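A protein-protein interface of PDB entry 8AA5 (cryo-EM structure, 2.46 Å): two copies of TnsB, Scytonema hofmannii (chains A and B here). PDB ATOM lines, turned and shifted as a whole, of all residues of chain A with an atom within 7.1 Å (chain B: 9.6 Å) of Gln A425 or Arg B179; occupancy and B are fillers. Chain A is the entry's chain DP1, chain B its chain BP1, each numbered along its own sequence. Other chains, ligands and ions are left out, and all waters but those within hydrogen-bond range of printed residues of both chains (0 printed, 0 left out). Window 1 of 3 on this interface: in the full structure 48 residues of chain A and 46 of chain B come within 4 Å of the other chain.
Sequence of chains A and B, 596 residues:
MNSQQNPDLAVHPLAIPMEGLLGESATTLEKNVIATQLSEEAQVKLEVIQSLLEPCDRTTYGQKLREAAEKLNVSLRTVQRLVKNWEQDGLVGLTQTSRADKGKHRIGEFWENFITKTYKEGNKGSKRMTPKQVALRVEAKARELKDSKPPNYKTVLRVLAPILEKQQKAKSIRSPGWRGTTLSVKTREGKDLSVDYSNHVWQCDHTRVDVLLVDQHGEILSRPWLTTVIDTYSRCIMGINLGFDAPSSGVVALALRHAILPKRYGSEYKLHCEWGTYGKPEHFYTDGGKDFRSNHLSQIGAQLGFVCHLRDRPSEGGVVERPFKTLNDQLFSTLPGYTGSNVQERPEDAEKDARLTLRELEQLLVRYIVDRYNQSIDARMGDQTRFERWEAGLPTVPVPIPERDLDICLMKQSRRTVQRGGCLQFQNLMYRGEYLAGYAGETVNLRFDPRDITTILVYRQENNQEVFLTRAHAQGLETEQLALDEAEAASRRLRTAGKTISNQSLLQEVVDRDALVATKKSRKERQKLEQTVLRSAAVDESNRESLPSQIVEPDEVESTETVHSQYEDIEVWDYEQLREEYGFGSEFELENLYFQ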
ATOM      1  N   ARG A 416      36.040  -0.171 -23.075  1.00  0.00           N
ATOM      2  CA  ARG A 416      35.265  -1.401 -22.992  1.00  0.00           C
ATOM      3  C   ARG A 416      35.891  -2.295 -21.936  1.00  0.00           C
ATOM      4  O   ARG A 416      37.056  -2.685 -22.064  1.00  0.00           O
ATOM      5  CB  ARG A 416      35.216  -2.114 -24.343  1.00  0.00           C
ATOM      6  CG  ARG A 416      34.002  -1.761 -25.179  1.00  0.00           C
ATOM      7  CD  ARG A 416      32.709  -2.012 -24.419  1.00  0.00           C
ATOM      8  NE  ARG A 416      31.540  -1.779 -25.256  1.00  0.00           N
ATOM      9  CZ  ARG A 416      31.099  -0.580 -25.608  1.00  0.00           C
ATOM     10  NH1 ARG A 416      31.693   0.525 -25.192  1.00  0.00           N
ATOM     11  NH2 ARG A 416      30.034  -0.488 -26.400  1.00  0.00           N
ATOM     12  N   THR A 417      35.123  -2.618 -20.903  1.00  0.00           N
ATOM     13  CA  THR A 417      35.632  -3.409 -19.791  1.00  0.00           C
ATOM     14  C   THR A 417      35.616  -4.885 -20.166  1.00  0.00           C
ATOM     15  O   THR A 417      34.567  -5.432 -20.520  1.00  0.00           O
ATOM     16  CB  THR A 417      34.799  -3.160 -18.537  1.00  0.00           C
ATOM     17  OG1 THR A 417      35.237  -1.952 -17.905  1.00  0.00           O
ATOM     18  CG2 THR A 417      34.947  -4.312 -17.555  1.00  0.00           C
ATOM     19  N   VAL A 418      36.777  -5.526 -20.097  1.00  0.00           N
ATOM     20  CA  VAL A 418      36.865  -6.966 -20.305  1.00  0.00           C
ATOM     21  C   VAL A 418      36.446  -7.665 -19.022  1.00  0.00           C
ATOM     22  O   VAL A 418      36.977  -7.382 -17.942  1.00  0.00           O
ATOM     23  CB  VAL A 418      38.283  -7.375 -20.727  1.00  0.00           C
ATOM     24  CG1 VAL A 418      38.362  -8.876 -20.923  1.00  0.00           C
ATOM     25  CG2 VAL A 418      38.676  -6.657 -21.995  1.00  0.00           C
ATOM     26  N   GLN A 419      35.488  -8.573 -19.136  1.00  0.00           N
ATOM     27  CA  GLN A 419      34.907  -9.239 -17.985  1.00  0.00           C
ATOM     28  C   GLN A 419      35.565 -10.600 -17.779  1.00  0.00           C
ATOM     29  O   GLN A 419      36.516 -10.973 -18.468  1.00  0.00           O
ATOM     30  CB  GLN A 419      33.393  -9.348 -18.157  1.00  0.00           C
ATOM     31  CG  GLN A 419      32.739  -8.015 -18.474  1.00  0.00           C
ATOM     32  CD  GLN A 419      31.281  -8.144 -18.837  1.00  0.00           C
ATOM     33  OE1 GLN A 419      30.554  -8.943 -18.256  1.00  0.00           O
ATOM     34  NE2 GLN A 419      30.841  -7.351 -19.801  1.00  0.00           N
ATOM     35  N   CYS A 423      35.741 -11.706 -21.875  1.00  0.00           N
ATOM     36  CA  CYS A 423      34.551 -11.459 -22.672  1.00  0.00           C
ATOM     37  C   CYS A 423      34.251  -9.971 -22.693  1.00  0.00           C
ATOM     38  O   CYS A 423      34.606  -9.232 -21.772  1.00  0.00           O
ATOM     39  CB  CYS A 423      33.333 -12.226 -22.142  1.00  0.00           C
ATOM     40  SG  CYS A 423      33.110 -12.136 -20.363  1.00  0.00           S
ATOM     41  N   LEU A 424      33.594  -9.539 -23.764  1.00  0.00           N
ATOM     42  CA  LEU A 424      33.199  -8.153 -23.943  1.00  0.00           C
ATOM     43  C   LEU A 424      31.712  -8.095 -24.240  1.00  0.00           C
ATOM     44  O   LEU A 424      31.146  -9.011 -24.841  1.00  0.00           O
ATOM     45  CB  LEU A 424      33.973  -7.481 -25.084  1.00  0.00           C
ATOM     46  CG  LEU A 424      35.444  -7.159 -24.842  1.00  0.00           C
ATOM     47  CD1 LEU A 424      36.286  -7.637 -26.002  1.00  0.00           C
ATOM     48  CD2 LEU A 424      35.619  -5.674 -24.630  1.00  0.00           C
ATOM     49  N   GLN A 425      31.084  -7.012 -23.815  1.00  0.00           N
ATOM     50  CA  GLN A 425      29.663  -6.788 -24.043  1.00  0.00           C
ATOM     51  C   GLN A 425      29.543  -5.663 -25.063  1.00  0.00           C
ATOM     52  O   GLN A 425      29.681  -4.485 -24.724  1.00  0.00           O
ATOM     53  CB  GLN A 425      28.955  -6.464 -22.731  1.00  0.00           C
ATOM     54  CG  GLN A 425      27.491  -6.854 -22.701  1.00  0.00           C
ATOM     55  CD  GLN A 425      26.585  -5.659 -22.810  1.00  0.00           C
ATOM     56  OE1 GLN A 425      26.821  -4.774 -23.618  1.00  0.00           O
ATOM     57  NE2 GLN A 425      25.542  -5.626 -21.995  1.00  0.00           N
ATOM     58  N   PHE A 426      29.291  -6.033 -26.317  1.00  0.00           N
ATOM     59  CA  PHE A 426      29.242  -5.088 -27.428  1.00  0.00           C
ATOM     60  C   PHE A 426      27.933  -5.271 -28.179  1.00  0.00           C
ATOM     61  O   PHE A 426      27.631  -6.375 -28.642  1.00  0.00           O
ATOM     62  CB  PHE A 426      30.436  -5.289 -28.366  1.00  0.00           C
ATOM     63  CG  PHE A 426      30.427  -4.387 -29.563  1.00  0.00           C
ATOM     64  CD1 PHE A 426      30.411  -3.014 -29.411  1.00  0.00           C
ATOM     65  CD2 PHE A 426      30.436  -4.914 -30.840  1.00  0.00           C
ATOM     66  CE1 PHE A 426      30.400  -2.186 -30.512  1.00  0.00           C
ATOM     67  CE2 PHE A 426      30.424  -4.091 -31.942  1.00  0.00           C
ATOM     68  CZ  PHE A 426      30.407  -2.725 -31.778  1.00  0.00           C
ATOM     69  N   GLN A 427      27.169  -4.186 -28.305  1.00  0.00           N
ATOM     70  CA  GLN A 427      25.893  -4.176 -29.019  1.00  0.00           C
ATOM     71  C   GLN A 427      24.955  -5.265 -28.502  1.00  0.00           C
ATOM     72  O   GLN A 427      24.362  -6.027 -29.269  1.00  0.00           O
ATOM     73  CB  GLN A 427      26.105  -4.310 -30.529  1.00  0.00           C
ATOM     74  CG  GLN A 427      26.690  -3.088 -31.259  1.00  0.00           C
ATOM     75  CD  GLN A 427      26.170  -1.729 -30.798  1.00  0.00           C
ATOM     76  OE1 GLN A 427      25.113  -1.612 -30.176  1.00  0.00           O
ATOM     77  NE2 GLN A 427      26.927  -0.685 -31.112  1.00  0.00           N
ATOM     78  N   ASN A 428      24.832  -5.333 -27.176  1.00  0.00           N
ATOM     79  CA  ASN A 428      23.944  -6.281 -26.501  1.00  0.00           C
ATOM     80  C   ASN A 428      24.283  -7.725 -26.852  1.00  0.00           C
ATOM     81  O   ASN A 428      23.408  -8.593 -26.875  1.00  0.00           O
ATOM     82  CB  ASN A 428      22.475  -5.981 -26.809  1.00  0.00           C
ATOM     83  CG  ASN A 428      22.021  -4.659 -26.230  1.00  0.00           C
ATOM     84  OD1 ASN A 428      21.667  -3.737 -26.961  1.00  0.00           O
ATOM     85  ND2 ASN A 428      22.031  -4.560 -24.908  1.00  0.00           N
ATOM     86  N   LEU A 429      25.554  -7.991 -27.128  1.00  0.00           N
ATOM     87  CA  LEU A 429      26.044  -9.333 -27.390  1.00  0.00           C
ATOM     88  C   LEU A 429      27.333  -9.544 -26.616  1.00  0.00           C
ATOM     89  O   LEU A 429      28.050  -8.594 -26.292  1.00  0.00           O
ATOM     90  CB  LEU A 429      26.291  -9.574 -28.884  1.00  0.00           C
ATOM     91  CG  LEU A 429      25.130  -9.319 -29.841  1.00  0.00           C
ATOM     92  CD1 LEU A 429      25.630  -8.615 -31.085  1.00  0.00           C
ATOM     93  CD2 LEU A 429      24.432 -10.618 -30.197  1.00  0.00           C
ATOM     94  N   MET A 430      27.625 -10.804 -26.321  1.00  0.00           N
ATOM     95  CA  MET A 430      28.833 -11.169 -25.600  1.00  0.00           C
ATOM     96  C   MET A 430      29.879 -11.644 -26.599  1.00  0.00           C
ATOM     97  O   MET A 430      29.632 -12.580 -27.366  1.00  0.00           O
ATOM     98  CB  MET A 430      28.546 -12.247 -24.557  1.00  0.00           C
ATOM     99  CG  MET A 430      29.279 -12.018 -23.255  1.00  0.00           C
ATOM    100  SD  MET A 430      28.873 -10.412 -22.551  1.00  0.00           S
ATOM    101  CE  MET A 430      30.329 -10.105 -21.563  1.00  0.00           C
ATOM    102  N   TYR A 431      31.038 -10.994 -26.590  1.00  0.00           N
ATOM    103  CA  TYR A 431      32.129 -11.297 -27.504  1.00  0.00           C
ATOM    104  C   TYR A 431      33.271 -11.936 -26.733  1.00  0.00           C
ATOM    105  O   TYR A 431      33.693 -11.414 -25.699  1.00  0.00           O
ATOM    106  CB  TYR A 431      32.616 -10.033 -28.210  1.00  0.00           C
ATOM    107  CG  TYR A 431      31.730  -9.581 -29.338  1.00  0.00           C
ATOM    108  CD1 TYR A 431      30.549  -8.901 -29.089  1.00  0.00           C
ATOM    109  CD2 TYR A 431      32.073  -9.834 -30.655  1.00  0.00           C
ATOM    110  CE1 TYR A 431      29.738  -8.486 -30.118  1.00  0.00           C
ATOM    111  CE2 TYR A 431      31.272  -9.424 -31.686  1.00  0.00           C
ATOM    112  CZ  TYR A 431      30.104  -8.751 -31.417  1.00  0.00           C
ATOM    113  OH  TYR A 431      29.297  -8.339 -32.452  1.00  0.00           O
ATOM    114  N   LEU A 446      37.904  -1.179 -29.167  1.00  0.00           N
ATOM    115  CA  LEU A 446      37.202  -2.047 -30.100  1.00  0.00           C
ATOM    116  C   LEU A 446      37.287  -1.468 -31.503  1.00  0.00           C
ATOM    117  O   LEU A 446      36.978  -0.291 -31.713  1.00  0.00           O
ATOM    118  CB  LEU A 446      35.736  -2.223 -29.699  1.00  0.00           C
ATOM    119  CG  LEU A 446      35.419  -3.166 -28.541  1.00  0.00           C
ATOM    120  CD1 LEU A 446      33.948  -3.533 -28.556  1.00  0.00           C
ATOM    121  CD2 LEU A 446      36.288  -4.408 -28.605  1.00  0.00           C
ATOM    122  N   ILE A 456      35.143  -8.863 -34.080  1.00  0.00           N
ATOM    123  CA  ILE A 456      35.616  -7.520 -33.780  1.00  0.00           C
ATOM    124  C   ILE A 456      37.059  -7.618 -33.306  1.00  0.00           C
ATOM    125  O   ILE A 456      37.533  -8.679 -32.897  1.00  0.00           O
ATOM    126  CB  ILE A 456      34.747  -6.803 -32.725  1.00  0.00           C
ATOM    127  CG1 ILE A 456      34.786  -7.552 -31.396  1.00  0.00           C
ATOM    128  CG2 ILE A 456      33.318  -6.669 -33.213  1.00  0.00           C
ATOM    129  CD1 ILE A 456      34.053  -6.850 -30.285  1.00  0.00           C
ATOM    130  N   ARG B 174      33.964  -8.055 -13.264  1.00  0.00           N
ATOM    131  CA  ARG B 174      32.542  -8.270 -13.487  1.00  0.00           C
ATOM    132  C   ARG B 174      32.312  -9.600 -14.193  1.00  0.00           C
ATOM    133  O   ARG B 174      33.109 -10.010 -15.040  1.00  0.00           O
ATOM    134  CB  ARG B 174      31.958  -7.127 -14.318  1.00  0.00           C
ATOM    135  CG  ARG B 174      30.454  -7.142 -14.475  1.00  0.00           C
ATOM    136  CD  ARG B 174      30.032  -6.178 -15.562  1.00  0.00           C
ATOM    137  NE  ARG B 174      28.643  -5.760 -15.429  1.00  0.00           N
ATOM    138  CZ  ARG B 174      27.602  -6.478 -15.823  1.00  0.00           C
ATOM    139  NH1 ARG B 174      27.755  -7.666 -16.382  1.00  0.00           N
ATOM    140  NH2 ARG B 174      26.378  -5.990 -15.658  1.00  0.00           N
ATOM    141  N   SER B 175      31.218 -10.275 -13.831  1.00  0.00           N
ATOM    142  CA  SER B 175      30.862 -11.562 -14.420  1.00  0.00           C
ATOM    143  C   SER B 175      29.818 -11.370 -15.506  1.00  0.00           C
ATOM    144  O   SER B 175      28.815 -10.680 -15.275  1.00  0.00           O
ATOM    145  CB  SER B 175      30.328 -12.511 -13.354  1.00  0.00           C
ATOM    146  OG  SER B 175      31.367 -13.315 -12.827  1.00  0.00           O
ATOM    147  N   PRO B 176      30.022 -11.944 -16.695  1.00  0.00           N
ATOM    148  CA  PRO B 176      29.053 -11.732 -17.783  1.00  0.00           C
ATOM    149  C   PRO B 176      27.655 -12.231 -17.473  1.00  0.00           C
ATOM    150  O   PRO B 176      26.674 -11.596 -17.878  1.00  0.00           O
ATOM    151  CB  PRO B 176      29.684 -12.496 -18.954  1.00  0.00           C
ATOM    152  CG  PRO B 176      30.571 -13.505 -18.312  1.00  0.00           C
ATOM    153  CD  PRO B 176      31.121 -12.834 -17.099  1.00  0.00           C
ATOM    154  N   GLY B 177      27.529 -13.351 -16.771  1.00  0.00           N
ATOM    155  CA  GLY B 177      26.235 -13.932 -16.493  1.00  0.00           C
ATOM    156  C   GLY B 177      25.675 -14.691 -17.682  1.00  0.00           C
ATOM    157  O   GLY B 177      26.202 -14.660 -18.794  1.00  0.00           O
ATOM    158  N   TRP B 178      24.573 -15.391 -17.432  1.00  0.00           N
ATOM    159  CA  TRP B 178      23.909 -16.149 -18.479  1.00  0.00           C
ATOM    160  C   TRP B 178      23.114 -15.223 -19.390  1.00  0.00           C
ATOM    161  O   TRP B 178      22.575 -14.200 -18.958  1.00  0.00           O
ATOM    162  CB  TRP B 178      22.977 -17.199 -17.881  1.00  0.00           C
ATOM    163  CG  TRP B 178      23.665 -18.420 -17.366  1.00  0.00           C
ATOM    164  CD1 TRP B 178      24.191 -18.599 -16.123  1.00  0.00           C
ATOM    165  CD2 TRP B 178      23.881 -19.647 -18.072  1.00  0.00           C
ATOM    166  NE1 TRP B 178      24.729 -19.855 -16.013  1.00  0.00           N
ATOM    167  CE2 TRP B 178      24.551 -20.519 -17.196  1.00  0.00           C
ATOM    168  CE3 TRP B 178      23.575 -20.089 -19.361  1.00  0.00           C
ATOM    169  CZ2 TRP B 178      24.922 -21.806 -17.568  1.00  0.00           C
ATOM    170  CZ3 TRP B 178      23.945 -21.366 -19.726  1.00  0.00           C
ATOM    171  CH2 TRP B 178      24.611 -22.209 -18.834  1.00  0.00           C
ATOM    172  N   ARG B 179      23.046 -15.593 -20.664  1.00  0.00           N
ATOM    173  CA  ARG B 179      22.264 -14.869 -21.653  1.00  0.00           C
ATOM    174  C   ARG B 179      21.300 -15.822 -22.342  1.00  0.00           C
ATOM    175  O   ARG B 179      21.591 -17.010 -22.513  1.00  0.00           O
ATOM    176  CB  ARG B 179      23.160 -14.196 -22.700  1.00  0.00           C
ATOM    177  CG  ARG B 179      24.518 -13.767 -22.184  1.00  0.00           C
ATOM    178  CD  ARG B 179      24.520 -12.301 -21.801  1.00  0.00           C
ATOM    179  NE  ARG B 179      24.442 -11.435 -22.970  1.00  0.00           N
ATOM    180  CZ  ARG B 179      24.465 -10.111 -22.922  1.00  0.00           C
ATOM    181  NH1 ARG B 179      24.570  -9.463 -21.775  1.00  0.00           N
ATOM    182  NH2 ARG B 179      24.380  -9.419 -24.055  1.00  0.00           N
ATOM    183  N   GLY B 180      20.147 -15.295 -22.731  1.00  0.00           N
ATOM    184  CA  GLY B 180      19.186 -16.083 -23.470  1.00  0.00           C
ATOM    185  C   GLY B 180      18.340 -16.978 -22.582  1.00  0.00           C
ATOM    186  O   GLY B 180      18.281 -16.834 -21.358  1.00  0.00           O
ATOM    187  N   THR B 181      17.668 -17.925 -23.234  1.00  0.00           N
ATOM    188  CA  THR B 181      16.722 -18.806 -22.562  1.00  0.00           C
ATOM    189  C   THR B 181      17.394 -20.006 -21.909  1.00  0.00           C
ATOM    190  O   THR B 181      16.968 -20.440 -20.835  1.00  0.00           O
ATOM    191  CB  THR B 181      15.659 -19.288 -23.552  1.00  0.00           C
ATOM    192  OG1 THR B 181      15.385 -18.252 -24.504  1.00  0.00           O
ATOM    193  CG2 THR B 181      14.376 -19.644 -22.822  1.00  0.00           C
ATOM    194  N   THR B 182      18.431 -20.556 -22.534  1.00  0.00           N
ATOM    195  CA  THR B 182      19.105 -21.716 -21.970  1.00  0.00           C
ATOM    196  C   THR B 182      19.810 -21.345 -20.671  1.00  0.00           C
ATOM    197  O   THR B 182      20.310 -20.230 -20.501  1.00  0.00           O
ATOM    198  CB  THR B 182      20.099 -22.304 -22.977  1.00  0.00           C
ATOM    199  OG1 THR B 182      20.519 -23.601 -22.538  1.00  0.00           O
ATOM    200  CG2 THR B 182      21.316 -21.404 -23.147  1.00  0.00           C
ATOM    201  N   LEU B 183      19.818 -22.288 -19.734  1.00  0.00           N
ATOM    202  CA  LEU B 183      20.355 -22.024 -18.409  1.00  0.00           C
ATOM    203  C   LEU B 183      20.638 -23.342 -17.710  1.00  0.00           C
ATOM    204  O   LEU B 183      19.869 -24.297 -17.837  1.00  0.00           O
ATOM    205  CB  LEU B 183      19.384 -21.177 -17.579  1.00  0.00           C
ATOM    206  CG  LEU B 183      19.714 -20.966 -16.102  1.00  0.00           C
ATOM    207  CD1 LEU B 183      20.995 -20.171 -15.946  1.00  0.00           C
ATOM    208  CD2 LEU B 183      18.565 -20.276 -15.394  1.00  0.00           C
ATOM    209  N   SER B 184      21.748 -23.383 -16.979  1.00  0.00           N
ATOM    210  CA  SER B 184      22.098 -24.518 -16.143  1.00  0.00           C
ATOM    211  C   SER B 184      22.656 -24.001 -14.827  1.00  0.00           C
ATOM    212  O   SER B 184      23.209 -22.901 -14.761  1.00  0.00           O
ATOM    213  CB  SER B 184      23.119 -25.434 -16.824  1.00  0.00           C
ATOM    214  OG  SER B 184      22.498 -26.260 -17.793  1.00  0.00           O
ATOM    215  N   ARG B 235      12.288 -16.800 -12.977  1.00  0.00           N
ATOM    216  CA  ARG B 235      12.680 -15.789 -11.997  1.00  0.00           C
ATOM    217  C   ARG B 235      11.473 -15.160 -11.304  1.00  0.00           C
ATOM    218  O   ARG B 235      11.574 -14.065 -10.745  1.00  0.00           O
ATOM    219  CB  ARG B 235      13.560 -14.706 -12.633  1.00  0.00           C
ATOM    220  CG  ARG B 235      15.048 -15.016 -12.598  1.00  0.00           C
ATOM    221  CD  ARG B 235      15.427 -16.104 -13.589  1.00  0.00           C
ATOM    222  NE  ARG B 235      15.216 -15.692 -14.971  1.00  0.00           N
ATOM    223  CZ  ARG B 235      15.483 -16.448 -16.028  1.00  0.00           C
ATOM    224  NH1 ARG B 235      15.982 -17.665 -15.896  1.00  0.00           N
ATOM    225  NH2 ARG B 235      15.242 -15.972 -17.245  1.00  0.00           N
ATOM    226  N   ALA B 379      14.866  -9.648 -16.724  1.00  0.00           N
ATOM    227  CA  ALA B 379      15.913  -8.856 -17.362  1.00  0.00           C
ATOM    228  C   ALA B 379      16.727  -9.671 -18.356  1.00  0.00           C
ATOM    229  O   ALA B 379      17.293  -9.110 -19.300  1.00  0.00           O
ATOM    230  CB  ALA B 379      16.828  -8.245 -16.303  1.00  0.00           C
ATOM    231  N   ARG B 380      16.805 -10.988 -18.160  1.00  0.00           N
ATOM    232  CA  ARG B 380      17.532 -11.835 -19.100  1.00  0.00           C
ATOM    233  C   ARG B 380      16.889 -11.810 -20.481  1.00  0.00           C
ATOM    234  O   ARG B 380      17.588 -11.751 -21.498  1.00  0.00           O
ATOM    235  CB  ARG B 380      17.593 -13.263 -18.566  1.00  0.00           C
ATOM    236  CG  ARG B 380      18.725 -14.088 -19.119  1.00  0.00           C
ATOM    237  CD  ARG B 380      18.945 -15.315 -18.264  1.00  0.00           C
ATOM    238  NE  ARG B 380      18.826 -15.012 -16.844  1.00  0.00           N
ATOM    239  CZ  ARG B 380      19.214 -15.825 -15.872  1.00  0.00           C
ATOM    240  NH1 ARG B 380      19.747 -17.005 -16.132  1.00  0.00           N
ATOM    241  NH2 ARG B 380      19.061 -15.444 -14.608  1.00  0.00           N
ATOM    242  N   MET B 381      15.559 -11.857 -20.535  1.00  0.00           N
ATOM    243  CA  MET B 381      14.839 -11.881 -21.802  1.00  0.00           C
ATOM    244  C   MET B 381      14.486 -10.480 -22.286  1.00  0.00           C
ATOM    245  O   MET B 381      14.704 -10.152 -23.456  1.00  0.00           O
ATOM    246  CB  MET B 381      13.576 -12.734 -21.665  1.00  0.00           C
ATOM    247  CG  MET B 381      13.831 -14.115 -21.091  1.00  0.00           C
ATOM    248  SD  MET B 381      14.969 -15.081 -22.099  1.00  0.00           S
ATOM    249  CE  MET B 381      14.166 -14.996 -23.695  1.00  0.00           C
ATOM    250  N   ARG B 389       6.279 -15.337 -18.051  1.00  0.00           N
ATOM    251  CA  ARG B 389       7.239 -16.376 -18.400  1.00  0.00           C
ATOM    252  C   ARG B 389       6.939 -17.671 -17.662  1.00  0.00           C
ATOM    253  O   ARG B 389       7.054 -18.761 -18.233  1.00  0.00           O
ATOM    254  CB  ARG B 389       8.657 -15.898 -18.096  1.00  0.00           C
ATOM    255  CG  ARG B 389       9.729 -16.935 -18.353  1.00  0.00           C
ATOM    256  CD  ARG B 389      11.093 -16.291 -18.505  1.00  0.00           C
ATOM    257  NE  ARG B 389      12.166 -17.279 -18.531  1.00  0.00           N
ATOM    258  CZ  ARG B 389      12.607 -17.877 -19.629  1.00  0.00           C
ATOM    259  NH1 ARG B 389      12.090 -17.615 -20.816  1.00  0.00           N
ATOM    260  NH2 ARG B 389      13.594 -18.763 -19.531  1.00  0.00           N
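Of chain B, only Arg B179 comes within 4 Å of Gln A425. Arg B179 touches just these residues of chain A: Gln A425 (3.96 Å), Asn A428 (3.1 Å) and Leu A429 (3.6 Å). Of the printed residues of chain A, Ser B175 touches Gln A419. Of the printed residues of chain A, Arg B174 touches Gln A419 (3.2 Å). Of the printed residues of chain A, Pro B176 touches Gln A419 (3.2 Å), Cys A423 (3.5 Å) and Met A430 (3.6 Å). Printed residues of chain B within 4 Å of Gln A419: Arg B174 (3.2 Å), Ser B175 (3.7 Å) and Pro B176 (3.2 Å). Val A418 touches none of the printed residues of chain B. The nearest residue of chain B that does not touch Gln A425 is Arg B174 (6.4 Å). The nearest residue of chain A that does not touch Arg B179 is Met A430 (4.2 Å). The nearest printed residue of chain B that does not touch Asn A428 is Gly B180 (8.5 Å).
No position is printed for both chains. Of the 8 pairs that touch across the chains among the printed residues, none has its exchanged pair printed and touching as well.
Gln A419 touches Arg B174 (CB to O, 3.2 Å). OE1 of Gln A419 touches C of Ser B175, 3.7 Å away. Cys A423 touches Pro B176. Gln A425 touches Arg B179 (NE2 to NH1, 3.96 Å). Leu A429 touches Arg B179 (N to NH2, 3.6 Å). CB of Pro B176 touches CE of Met A430 (3.6 Å).
The guanidinium group (NE) of Arg A416 lies within hydrogen-bond range of the backbone carbonyl oxygen (O) of Gln A425 (3.3 Å).
NH2 of Arg B179 lies within hydrogen-bond range of O of Asn A428 (3.1 Å). The side-chain amide oxygen (OE1) of Gln A419 lies close to the backbone nitrogen (N) of Pro B176.
Of the 16 printed residues of chain B, 4 touch a printed residue of chain A. Hydrophobic or aromatic side chains of chain B that line the printed part of chain A: Pro B176. Printed residues of chain A that touch a printed residue of chain B: Gln A419, Cys A423, Gln A425, Asn A428, Leu A429 and Met A430. Hydrophobic or aromatic side chains of chain A within 4 Å of the printed part of chain B: Met A430. Among the printed residues, 8 pairs touch across the chains. Among the printed residues, no Asp or Glu carboxylate lies within 4 Å of a Lys or Arg side-chain nitrogen of the other chain.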
